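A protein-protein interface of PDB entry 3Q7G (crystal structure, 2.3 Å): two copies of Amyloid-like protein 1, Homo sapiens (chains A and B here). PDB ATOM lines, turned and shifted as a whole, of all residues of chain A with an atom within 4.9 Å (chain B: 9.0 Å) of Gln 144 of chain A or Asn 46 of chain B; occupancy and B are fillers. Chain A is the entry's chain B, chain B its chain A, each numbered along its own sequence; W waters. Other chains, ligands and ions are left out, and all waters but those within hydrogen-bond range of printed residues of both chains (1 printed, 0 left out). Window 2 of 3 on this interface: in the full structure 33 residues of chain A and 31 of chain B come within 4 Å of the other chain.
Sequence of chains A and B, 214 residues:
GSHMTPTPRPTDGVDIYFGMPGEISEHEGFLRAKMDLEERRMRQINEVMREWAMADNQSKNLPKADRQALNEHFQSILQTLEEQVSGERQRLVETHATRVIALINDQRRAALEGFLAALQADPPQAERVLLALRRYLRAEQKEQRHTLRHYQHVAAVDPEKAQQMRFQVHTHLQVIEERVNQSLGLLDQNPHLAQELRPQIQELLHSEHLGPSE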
ATOM      1  N   GLU A 140      36.372  -7.800  14.011  1.00  0.00           N
ATOM      2  CA  GLU A 140      35.019  -7.401  14.413  1.00  0.00           C
ATOM      3  C   GLU A 140      34.774  -7.676  15.902  1.00  0.00           C
ATOM      4  O   GLU A 140      34.148  -6.879  16.577  1.00  0.00           O
ATOM      5  CB  GLU A 140      33.964  -8.142  13.602  1.00  0.00           C
ATOM      6  CG  GLU A 140      33.848  -7.668  12.177  1.00  0.00           C
ATOM      7  CD  GLU A 140      33.381  -6.222  12.044  1.00  0.00           C
ATOM      8  OE1 GLU A 140      32.912  -5.889  10.938  1.00  0.00           O
ATOM      9  OE2 GLU A 140      33.483  -5.418  12.997  1.00  0.00           O
ATOM     10  N   GLN A 141      35.288  -8.808  16.391  1.00  0.00           N
ATOM     11  CA  GLN A 141      35.166  -9.192  17.793  1.00  0.00           C
ATOM     12  C   GLN A 141      35.916  -8.188  18.661  1.00  0.00           C
ATOM     13  O   GLN A 141      35.455  -7.818  19.748  1.00  0.00           O
ATOM     14  CB  GLN A 141      35.712 -10.634  18.019  1.00  0.00           C
ATOM     15  N   LYS A 142      37.071  -7.728  18.186  1.00  0.00           N
ATOM     16  CA  LYS A 142      37.811  -6.753  18.962  1.00  0.00           C
ATOM     17  C   LYS A 142      37.005  -5.463  19.040  1.00  0.00           C
ATOM     18  O   LYS A 142      37.069  -4.759  20.048  1.00  0.00           O
ATOM     19  CB  LYS A 142      39.191  -6.455  18.375  1.00  0.00           C
ATOM     20  CG  LYS A 142      40.039  -5.638  19.346  1.00  0.00           C
ATOM     21  CD  LYS A 142      41.517  -5.604  18.970  1.00  0.00           C
ATOM     22  CE  LYS A 142      42.360  -4.944  20.073  1.00  0.00           C
ATOM     23  NZ  LYS A 142      42.535  -5.778  21.301  1.00  0.00           N
ATOM     24  N   GLU A 143      36.262  -5.125  17.988  1.00  0.00           N
ATOM     25  CA  GLU A 143      35.459  -3.908  18.083  1.00  0.00           C
ATOM     26  C   GLU A 143      34.318  -4.172  19.081  1.00  0.00           C
ATOM     27  O   GLU A 143      33.920  -3.274  19.831  1.00  0.00           O
ATOM     28  CB  GLU A 143      34.883  -3.468  16.730  1.00  0.00           C
ATOM     29  CG  GLU A 143      34.365  -2.038  16.782  1.00  0.00           C
ATOM     30  CD  GLU A 143      33.818  -1.533  15.460  1.00  0.00           C
ATOM     31  OE1 GLU A 143      34.315  -1.967  14.401  1.00  0.00           O
ATOM     32  OE2 GLU A 143      32.904  -0.678  15.486  1.00  0.00           O
ATOM     33  N   GLN A 144      33.807  -5.406  19.080  1.00  0.00           N
ATOM     34  CA  GLN A 144      32.746  -5.790  20.006  1.00  0.00           C
ATOM     35  C   GLN A 144      33.239  -5.697  21.463  1.00  0.00           C
ATOM     36  O   GLN A 144      32.576  -5.086  22.301  1.00  0.00           O
ATOM     37  CB  GLN A 144      32.245  -7.208  19.733  1.00  0.00           C
ATOM     38  CG  GLN A 144      30.963  -7.518  20.475  1.00  0.00           C
ATOM     39  CD  GLN A 144      30.588  -8.988  20.454  1.00  0.00           C
ATOM     40  OE1 GLN A 144      31.291  -9.828  21.024  1.00  0.00           O
ATOM     41  NE2 GLN A 144      29.479  -9.310  19.798  1.00  0.00           N
ATOM     42  N   ARG A 145      34.403  -6.271  21.758  1.00  0.00           N
ATOM     43  CA  ARG A 145      34.948  -6.196  23.109  1.00  0.00           C
ATOM     44  C   ARG A 145      35.103  -4.746  23.514  1.00  0.00           C
ATOM     45  O   ARG A 145      34.644  -4.326  24.585  1.00  0.00           O
ATOM     46  CB  ARG A 145      36.306  -6.879  23.196  1.00  0.00           C
ATOM     47  CG  ARG A 145      36.232  -8.387  23.232  1.00  0.00           C
ATOM     48  N   HIS A 146      35.746  -3.976  22.650  1.00  0.00           N
ATOM     49  CA  HIS A 146      35.984  -2.575  22.943  1.00  0.00           C
ATOM     50  C   HIS A 146      34.690  -1.821  23.263  1.00  0.00           C
ATOM     51  O   HIS A 146      34.627  -1.053  24.237  1.00  0.00           O
ATOM     52  CB  HIS A 146      36.740  -1.940  21.776  1.00  0.00           C
ATOM     53  CG  HIS A 146      37.145  -0.524  22.010  1.00  0.00           C
ATOM     54  ND1 HIS A 146      36.333   0.540  21.687  1.00  0.00           N
ATOM     55  CD2 HIS A 146      38.276   0.006  22.536  1.00  0.00           C
ATOM     56  CE1 HIS A 146      36.944   1.666  22.004  1.00  0.00           C
ATOM     57  NE2 HIS A 146      38.124   1.370  22.523  1.00  0.00           N
ATOM     58  N   THR A 147      33.647  -2.045  22.466  1.00  0.00           N
ATOM     59  CA  THR A 147      32.367  -1.395  22.711  1.00  0.00           C
ATOM     60  C   THR A 147      31.806  -1.770  24.108  1.00  0.00           C
ATOM     61  O   THR A 147      31.317  -0.902  24.836  1.00  0.00           O
ATOM     62  CB  THR A 147      31.341  -1.783  21.640  1.00  0.00           C
ATOM     63  OG1 THR A 147      31.860  -1.463  20.339  1.00  0.00           O
ATOM     64  CG2 THR A 147      30.052  -1.051  21.862  1.00  0.00           C
ATOM     65  N   LEU A 148      31.861  -3.054  24.467  1.00  0.00           N
ATOM     66  CA  LEU A 148      31.349  -3.527  25.752  1.00  0.00           C
ATOM     67  C   LEU A 148      32.199  -3.053  26.919  1.00  0.00           C
ATOM     68  O   LEU A 148      31.670  -2.690  27.970  1.00  0.00           O
ATOM     69  CB  LEU A 148      31.303  -5.056  25.778  1.00  0.00           C
ATOM     70  CG  LEU A 148      30.301  -5.795  24.888  1.00  0.00           C
ATOM     71  CD1 LEU A 148      30.774  -7.225  24.659  1.00  0.00           C
ATOM     72  CD2 LEU A 148      28.933  -5.805  25.528  1.00  0.00           C
ATOM     73  N   LEU A 173      26.396  -2.548  18.738  1.00  0.00           N
ATOM     74  CA  LEU A 173      26.598  -3.992  18.652  1.00  0.00           C
ATOM     75  C   LEU A 173      25.815  -4.537  17.463  1.00  0.00           C
ATOM     76  O   LEU A 173      26.285  -5.446  16.778  1.00  0.00           O
ATOM     77  CB  LEU A 173      26.135  -4.682  19.935  1.00  0.00           C
ATOM     78  CG  LEU A 173      26.990  -4.276  21.140  1.00  0.00           C
ATOM     79  CD1 LEU A 173      26.426  -4.844  22.481  1.00  0.00           C
ATOM     80  CD2 LEU A 173      28.420  -4.778  20.884  1.00  0.00           C
ATOM     81  N   ILE A 176      27.635  -3.766  14.281  1.00  0.00           N
ATOM     82  CA  ILE A 176      28.729  -4.706  14.089  1.00  0.00           C
ATOM     83  C   ILE A 176      28.225  -6.035  13.537  1.00  0.00           C
ATOM     84  O   ILE A 176      28.799  -6.567  12.574  1.00  0.00           O
ATOM     85  CB  ILE A 176      29.484  -4.948  15.393  1.00  0.00           C
ATOM     86  CG1 ILE A 176      30.115  -3.624  15.868  1.00  0.00           C
ATOM     87  CG2 ILE A 176      30.543  -6.038  15.201  1.00  0.00           C
ATOM     88  CD1 ILE A 176      30.668  -3.659  17.287  1.00  0.00           C
ATOM     89  N   GLU B  38      35.667  -7.055  35.538  1.00  0.00           N
ATOM     90  CA  GLU B  38      35.459  -6.404  34.234  1.00  0.00           C
ATOM     91  C   GLU B  38      35.050  -7.455  33.201  1.00  0.00           C
ATOM     92  O   GLU B  38      34.080  -7.265  32.471  1.00  0.00           O
ATOM     93  CB  GLU B  38      36.741  -5.688  33.792  1.00  0.00           C
ATOM     94  CG  GLU B  38      36.776  -5.191  32.348  1.00  0.00           C
ATOM     95  CD  GLU B  38      38.047  -4.397  32.045  1.00  0.00           C
ATOM     96  OE1 GLU B  38      37.978  -3.147  32.000  1.00  0.00           O
ATOM     97  OE2 GLU B  38      39.125  -5.021  31.876  1.00  0.00           O
ATOM     98  N   GLU B  39      35.785  -8.562  33.149  1.00  0.00           N
ATOM     99  CA  GLU B  39      35.476  -9.641  32.204  1.00  0.00           C
ATOM    100  C   GLU B  39      34.104 -10.257  32.516  1.00  0.00           C
ATOM    101  O   GLU B  39      33.265 -10.429  31.618  1.00  0.00           O
ATOM    102  CB  GLU B  39      36.551 -10.739  32.242  1.00  0.00           C
ATOM    103  CG  GLU B  39      37.932 -10.355  31.693  1.00  0.00           C
ATOM    104  CD  GLU B  39      37.913  -9.886  30.226  1.00  0.00           C
ATOM    105  OE1 GLU B  39      37.140 -10.457  29.415  1.00  0.00           O
ATOM    106  OE2 GLU B  39      38.682  -8.957  29.875  1.00  0.00           O
ATOM    107  N   ARG B  40      33.875 -10.586  33.785  1.00  0.00           N
ATOM    108  CA  ARG B  40      32.611 -11.180  34.211  1.00  0.00           C
ATOM    109  C   ARG B  40      31.437 -10.288  33.799  1.00  0.00           C
ATOM    110  O   ARG B  40      30.466 -10.747  33.188  1.00  0.00           O
ATOM    111  CB  ARG B  40      32.595 -11.362  35.739  1.00  0.00           C
ATOM    112  CG  ARG B  40      31.309 -11.980  36.304  1.00  0.00           C
ATOM    113  CD  ARG B  40      31.250 -11.937  37.839  1.00  0.00           C
ATOM    114  NE  ARG B  40      32.355 -12.653  38.477  1.00  0.00           N
ATOM    115  CZ  ARG B  40      32.612 -12.620  39.779  1.00  0.00           C
ATOM    116  NH1 ARG B  40      31.843 -11.905  40.592  1.00  0.00           N
ATOM    117  NH2 ARG B  40      33.641 -13.297  40.267  1.00  0.00           N
ATOM    118  N   ARG B  41      31.526  -9.005  34.119  1.00  0.00           N
ATOM    119  CA  ARG B  41      30.443  -8.091  33.804  1.00  0.00           C
ATOM    120  C   ARG B  41      30.265  -7.842  32.317  1.00  0.00           C
ATOM    121  O   ARG B  41      29.146  -7.621  31.860  1.00  0.00           O
ATOM    122  CB  ARG B  41      30.624  -6.764  34.554  1.00  0.00           C
ATOM    123  CG  ARG B  41      30.503  -6.918  36.068  1.00  0.00           C
ATOM    124  CD  ARG B  41      29.191  -7.592  36.479  1.00  0.00           C
ATOM    125  NE  ARG B  41      28.969  -7.518  37.920  1.00  0.00           N
ATOM    126  CZ  ARG B  41      27.844  -7.883  38.534  1.00  0.00           C
ATOM    127  NH1 ARG B  41      26.819  -8.359  37.839  1.00  0.00           N
ATOM    128  NH2 ARG B  41      27.735  -7.753  39.849  1.00  0.00           N
ATOM    129  N   MET B  42      31.362  -7.874  31.566  1.00  0.00           N
ATOM    130  CA  MET B  42      31.280  -7.686  30.126  1.00  0.00           C
ATOM    131  C   MET B  42      30.504  -8.856  29.533  1.00  0.00           C
ATOM    132  O   MET B  42      29.667  -8.668  28.646  1.00  0.00           O
ATOM    133  CB  MET B  42      32.676  -7.607  29.508  1.00  0.00           C
ATOM    134  CG  MET B  42      33.245  -6.207  29.501  1.00  0.00           C
ATOM    135  SD  MET B  42      35.021  -6.166  29.149  1.00  0.00           S
ATOM    136  CE  MET B  42      35.024  -6.773  27.454  1.00  0.00           C
ATOM    137  N   ARG B  43      30.760 -10.059  30.039  1.00  0.00           N
ATOM    138  CA  ARG B  43      30.062 -11.228  29.530  1.00  0.00           C
ATOM    139  C   ARG B  43      28.578 -11.147  29.832  1.00  0.00           C
ATOM    140  O   ARG B  43      27.765 -11.420  28.962  1.00  0.00           O
ATOM    141  CB  ARG B  43      30.658 -12.535  30.088  1.00  0.00           C
ATOM    142  CG  ARG B  43      31.875 -13.027  29.301  1.00  0.00           C
ATOM    143  CD  ARG B  43      32.262 -14.483  29.599  1.00  0.00           C
ATOM    144  NE  ARG B  43      33.320 -14.603  30.606  1.00  0.00           N
ATOM    145  CZ  ARG B  43      33.112 -14.682  31.918  1.00  0.00           C
ATOM    146  NH1 ARG B  43      31.876 -14.660  32.408  1.00  0.00           N
ATOM    147  NH2 ARG B  43      34.145 -14.770  32.748  1.00  0.00           N
ATOM    148  N   GLN B  44      28.228 -10.747  31.047  1.00  0.00           N
ATOM    149  CA  GLN B  44      26.813 -10.627  31.407  1.00  0.00           C
ATOM    150  C   GLN B  44      26.095  -9.646  30.472  1.00  0.00           C
ATOM    151  O   GLN B  44      25.058  -9.962  29.879  1.00  0.00           O
ATOM    152  CB  GLN B  44      26.650 -10.152  32.856  1.00  0.00           C
ATOM    153  CG  GLN B  44      27.238 -11.075  33.907  1.00  0.00           C
ATOM    154  CD  GLN B  44      26.881 -10.635  35.333  1.00  0.00           C
ATOM    155  OE1 GLN B  44      26.828  -9.439  35.628  1.00  0.00           O
ATOM    156  NE2 GLN B  44      26.645 -11.605  36.218  1.00  0.00           N
ATOM    157  N   ILE B  45      26.664  -8.450  30.351  1.00  0.00           N
ATOM    158  CA  ILE B  45      26.115  -7.399  29.503  1.00  0.00           C
ATOM    159  C   ILE B  45      25.969  -7.874  28.045  1.00  0.00           C
ATOM    160  O   ILE B  45      25.004  -7.532  27.355  1.00  0.00           O
ATOM    161  CB  ILE B  45      27.027  -6.155  29.567  1.00  0.00           C
ATOM    162  CG1 ILE B  45      27.024  -5.585  30.995  1.00  0.00           C
ATOM    163  CG2 ILE B  45      26.610  -5.141  28.512  1.00  0.00           C
ATOM    164  CD1 ILE B  45      27.997  -4.425  31.217  1.00  0.00           C
ATOM    165  N   ASN B  46      26.920  -8.670  27.576  1.00  0.00           N
ATOM    166  CA  ASN B  46      26.833  -9.145  26.204  1.00  0.00           C
ATOM    167  C   ASN B  46      25.636 -10.086  26.029  1.00  0.00           C
ATOM    168  O   ASN B  46      24.945 -10.030  25.004  1.00  0.00           O
ATOM    169  CB  ASN B  46      28.122  -9.837  25.771  1.00  0.00           C
ATOM    170  CG  ASN B  46      28.145 -10.122  24.272  1.00  0.00           C
ATOM    171  OD1 ASN B  46      27.914  -9.224  23.448  1.00  0.00           O
ATOM    172  ND2 ASN B  46      28.410 -11.373  23.913  1.00  0.00           N
ATOM    173  N   GLU B  47      25.385 -10.945  27.016  1.00  0.00           N
ATOM    174  CA  GLU B  47      24.244 -11.850  26.958  1.00  0.00           C
ATOM    175  C   GLU B  47      22.956 -11.003  26.895  1.00  0.00           C
ATOM    176  O   GLU B  47      22.101 -11.226  26.052  1.00  0.00           O
ATOM    177  CB  GLU B  47      24.186 -12.763  28.197  1.00  0.00           C
ATOM    178  CG  GLU B  47      25.094 -13.991  28.121  1.00  0.00           C
ATOM    179  CD  GLU B  47      24.912 -14.725  26.807  1.00  0.00           C
ATOM    180  OE1 GLU B  47      25.763 -14.528  25.900  1.00  0.00           O
ATOM    181  OE2 GLU B  47      23.898 -15.453  26.657  1.00  0.00           O
ATOM    182  N   VAL B  48      22.796 -10.040  27.794  1.00  0.00           N
ATOM    183  CA  VAL B  48      21.591  -9.221  27.737  1.00  0.00           C
ATOM    184  C   VAL B  48      21.460  -8.518  26.374  1.00  0.00           C
ATOM    185  O   VAL B  48      20.376  -8.509  25.790  1.00  0.00           O
ATOM    186  CB  VAL B  48      21.561  -8.141  28.823  1.00  0.00           C
ATOM    187  CG1 VAL B  48      20.265  -7.378  28.722  1.00  0.00           C
ATOM    188  CG2 VAL B  48      21.703  -8.763  30.203  1.00  0.00           C
ATOM    189  N   MET B  49      22.540  -7.926  25.867  1.00  0.00           N
ATOM    190  CA  MET B  49      22.462  -7.243  24.570  1.00  0.00           C
ATOM    191  C   MET B  49      22.059  -8.235  23.470  1.00  0.00           C
ATOM    192  O   MET B  49      21.280  -7.897  22.582  1.00  0.00           O
ATOM    193  CB  MET B  49      23.804  -6.584  24.206  1.00  0.00           C
ATOM    194  CG  MET B  49      24.218  -5.418  25.092  1.00  0.00           C
ATOM    195  SD  MET B  49      23.227  -3.940  24.790  1.00  0.00           S
ATOM    196  CE  MET B  49      23.666  -2.920  26.248  1.00  0.00           C
ATOM    197  N   ARG B  50      22.578  -9.457  23.528  1.00  0.00           N
ATOM    198  CA  ARG B  50      22.227 -10.454  22.519  1.00  0.00           C
ATOM    199  C   ARG B  50      20.732 -10.785  22.597  1.00  0.00           C
ATOM    200  O   ARG B  50      20.053 -10.874  21.567  1.00  0.00           O
ATOM    201  CB  ARG B  50      23.050 -11.713  22.716  1.00  0.00           C
ATOM    202  N   GLU B  51      20.224 -10.960  23.815  1.00  0.00           N
ATOM    203  CA  GLU B  51      18.811 -11.273  24.011  1.00  0.00           C
ATOM    204  C   GLU B  51      17.956 -10.115  23.532  1.00  0.00           C
ATOM    205  O   GLU B  51      16.902 -10.309  22.939  1.00  0.00           O
ATOM    206  CB  GLU B  51      18.505 -11.536  25.483  1.00  0.00           C
ATOM    207  CG  GLU B  51      19.196 -12.749  26.050  1.00  0.00           C
ATOM    208  CD  GLU B  51      18.886 -12.960  27.522  1.00  0.00           C
ATOM    209  OE1 GLU B  51      19.170 -12.051  28.336  1.00  0.00           O
ATOM    210  OE2 GLU B  51      18.358 -14.039  27.867  1.00  0.00           O
ATOM    211  N   TRP B  52      18.431  -8.905  23.784  1.00  0.00           N
ATOM    212  CA  TRP B  52      17.703  -7.717  23.388  1.00  0.00           C
ATOM    213  C   TRP B  52      17.682  -7.600  21.868  1.00  0.00           C
ATOM    214  O   TRP B  52      16.651  -7.281  21.300  1.00  0.00           O
ATOM    215  CB  TRP B  52      18.335  -6.489  24.033  1.00  0.00           C
ATOM    216  CG  TRP B  52      17.596  -5.208  23.831  1.00  0.00           C
ATOM    217  CD1 TRP B  52      16.343  -5.056  23.325  1.00  0.00           C
ATOM    218  CD2 TRP B  52      18.036  -3.896  24.213  1.00  0.00           C
ATOM    219  NE1 TRP B  52      15.968  -3.742  23.372  1.00  0.00           N
ATOM    220  CE2 TRP B  52      16.988  -3.004  23.915  1.00  0.00           C
ATOM    221  CE3 TRP B  52      19.210  -3.394  24.785  1.00  0.00           C
ATOM    222  CZ2 TRP B  52      17.071  -1.627  24.177  1.00  0.00           C
ATOM    223  CZ3 TRP B  52      19.300  -2.023  25.047  1.00  0.00           C
ATOM    224  CH2 TRP B  52      18.235  -1.158  24.744  1.00  0.00           C
ATOM    225  N   ALA B  53      18.803  -7.864  21.202  1.00  0.00           N
ATOM    226  CA  ALA B  53      18.830  -7.774  19.745  1.00  0.00           C
ATOM    227  C   ALA B  53      17.873  -8.807  19.175  1.00  0.00           C
ATOM    228  O   ALA B  53      17.069  -8.504  18.295  1.00  0.00           O
ATOM    229  CB  ALA B  53      20.225  -8.045  19.214  1.00  0.00           C
ATOM    230  N   MET B  54      17.972 -10.025  19.701  1.00  0.00           N
ATOM    231  CA  MET B  54      17.152 -11.151  19.267  1.00  0.00           C
ATOM    232  C   MET B  54      15.665 -10.871  19.451  1.00  0.00           C
ATOM    233  O   MET B  54      14.838 -11.324  18.658  1.00  0.00           O
ATOM    234  CB  MET B  54      17.538 -12.404  20.048  1.00  0.00           C
ATOM    235  CG  MET B  54      17.326 -13.700  19.297  1.00  0.00           C
ATOM    236  SD  MET B  54      17.700 -15.149  20.313  1.00  0.00           S
ATOM    237  CE  MET B  54      16.038 -15.631  20.819  1.00  0.00           C
ATOM    238  N   LEU B  78      19.133  -3.770  32.328  1.00  0.00           N
ATOM    239  CA  LEU B  78      20.438  -3.115  32.259  1.00  0.00           C
ATOM    240  C   LEU B  78      20.621  -2.083  33.379  1.00  0.00           C
ATOM    241  O   LEU B  78      21.721  -1.911  33.903  1.00  0.00           O
ATOM    242  CB  LEU B  78      20.635  -2.472  30.867  1.00  0.00           C
ATOM    243  CG  LEU B  78      20.777  -3.485  29.721  1.00  0.00           C
ATOM    244  CD1 LEU B  78      20.784  -2.817  28.344  1.00  0.00           C
ATOM    245  CD2 LEU B  78      22.074  -4.252  29.928  1.00  0.00           C
ATOM    246  N   LEU B  81      21.563  -4.100  36.119  1.00  0.00           N
ATOM    247  CA  LEU B  81      22.933  -4.549  35.918  1.00  0.00           C
ATOM    248  C   LEU B  81      23.943  -3.407  36.128  1.00  0.00           C
ATOM    249  O   LEU B  81      24.978  -3.606  36.756  1.00  0.00           O
ATOM    250  CB  LEU B  81      23.089  -5.139  34.527  1.00  0.00           C
ATOM    251  CG  LEU B  81      24.439  -5.776  34.224  1.00  0.00           C
ATOM    252  CD1 LEU B  81      24.857  -6.626  35.422  1.00  0.00           C
ATOM    253  CD2 LEU B  81      24.339  -6.598  32.919  1.00  0.00           C
HETATM  254  O   HOH W   1      26.554  -8.761  20.401  1.00  0.00           O
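Gln 144 of chain A touches Asn 46 of chain B. Arg 145 of chain A touches Met 42 of chain B. Ile 45 of chain B touches Leu 148 of chain A. CD1 of Leu 148 of chain A touches OD1 of Asn 46 of chain B, at 3.7 Å. Met 49 of chain B touches Leu 173 of chain A.
Of chain B, only Asn 46 (3.97 Å) comes within 4 Å of Gln 144 of chain A. Of chain B, only Met 42 comes within 4 Å of Arg 145 of chain A. Of the printed residues of chain B, Leu 148 of chain A touches Ile 45 and Asn 46. Printed residues of chain B within 4 Å of Leu 173 of chain A: Met 49. Printed residues of chain A within 4 Å of Met 42 of chain B: Arg 145. Of the printed residues of chain A, Met 49 of chain B touches Leu 173. The nearest residue of chain B that does not touch Gln 144 of chain A is Met 42 of chain B (5.9 Å). The nearest residue of chain A that does not touch Asn 46 of chain B is Leu 173 of chain A (4.7 Å).
Printed residues of chain A that touch a printed residue of chain B: Gln 144, Arg 145, Leu 148 and Leu 173. Along chain A the printed residues that touch a printed residue of chain B span positions 144 to 173. Printed residues of chain B that touch a printed residue of chain A: Met 42, Ile 45, Asn 46 and Met 49. Among the printed residues, 5 pairs touch across the chains. Among the printed residues, no Asp or Glu carboxylate lies within 4 Å of a Lys or Arg side-chain nitrogen of the other chain.
No position is printed for both chains.
Water W1 bridges the side-chain amide nitrogen of Gln 144 of chain A and the side-chain amide oxygen of Asn 46 of chain B.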
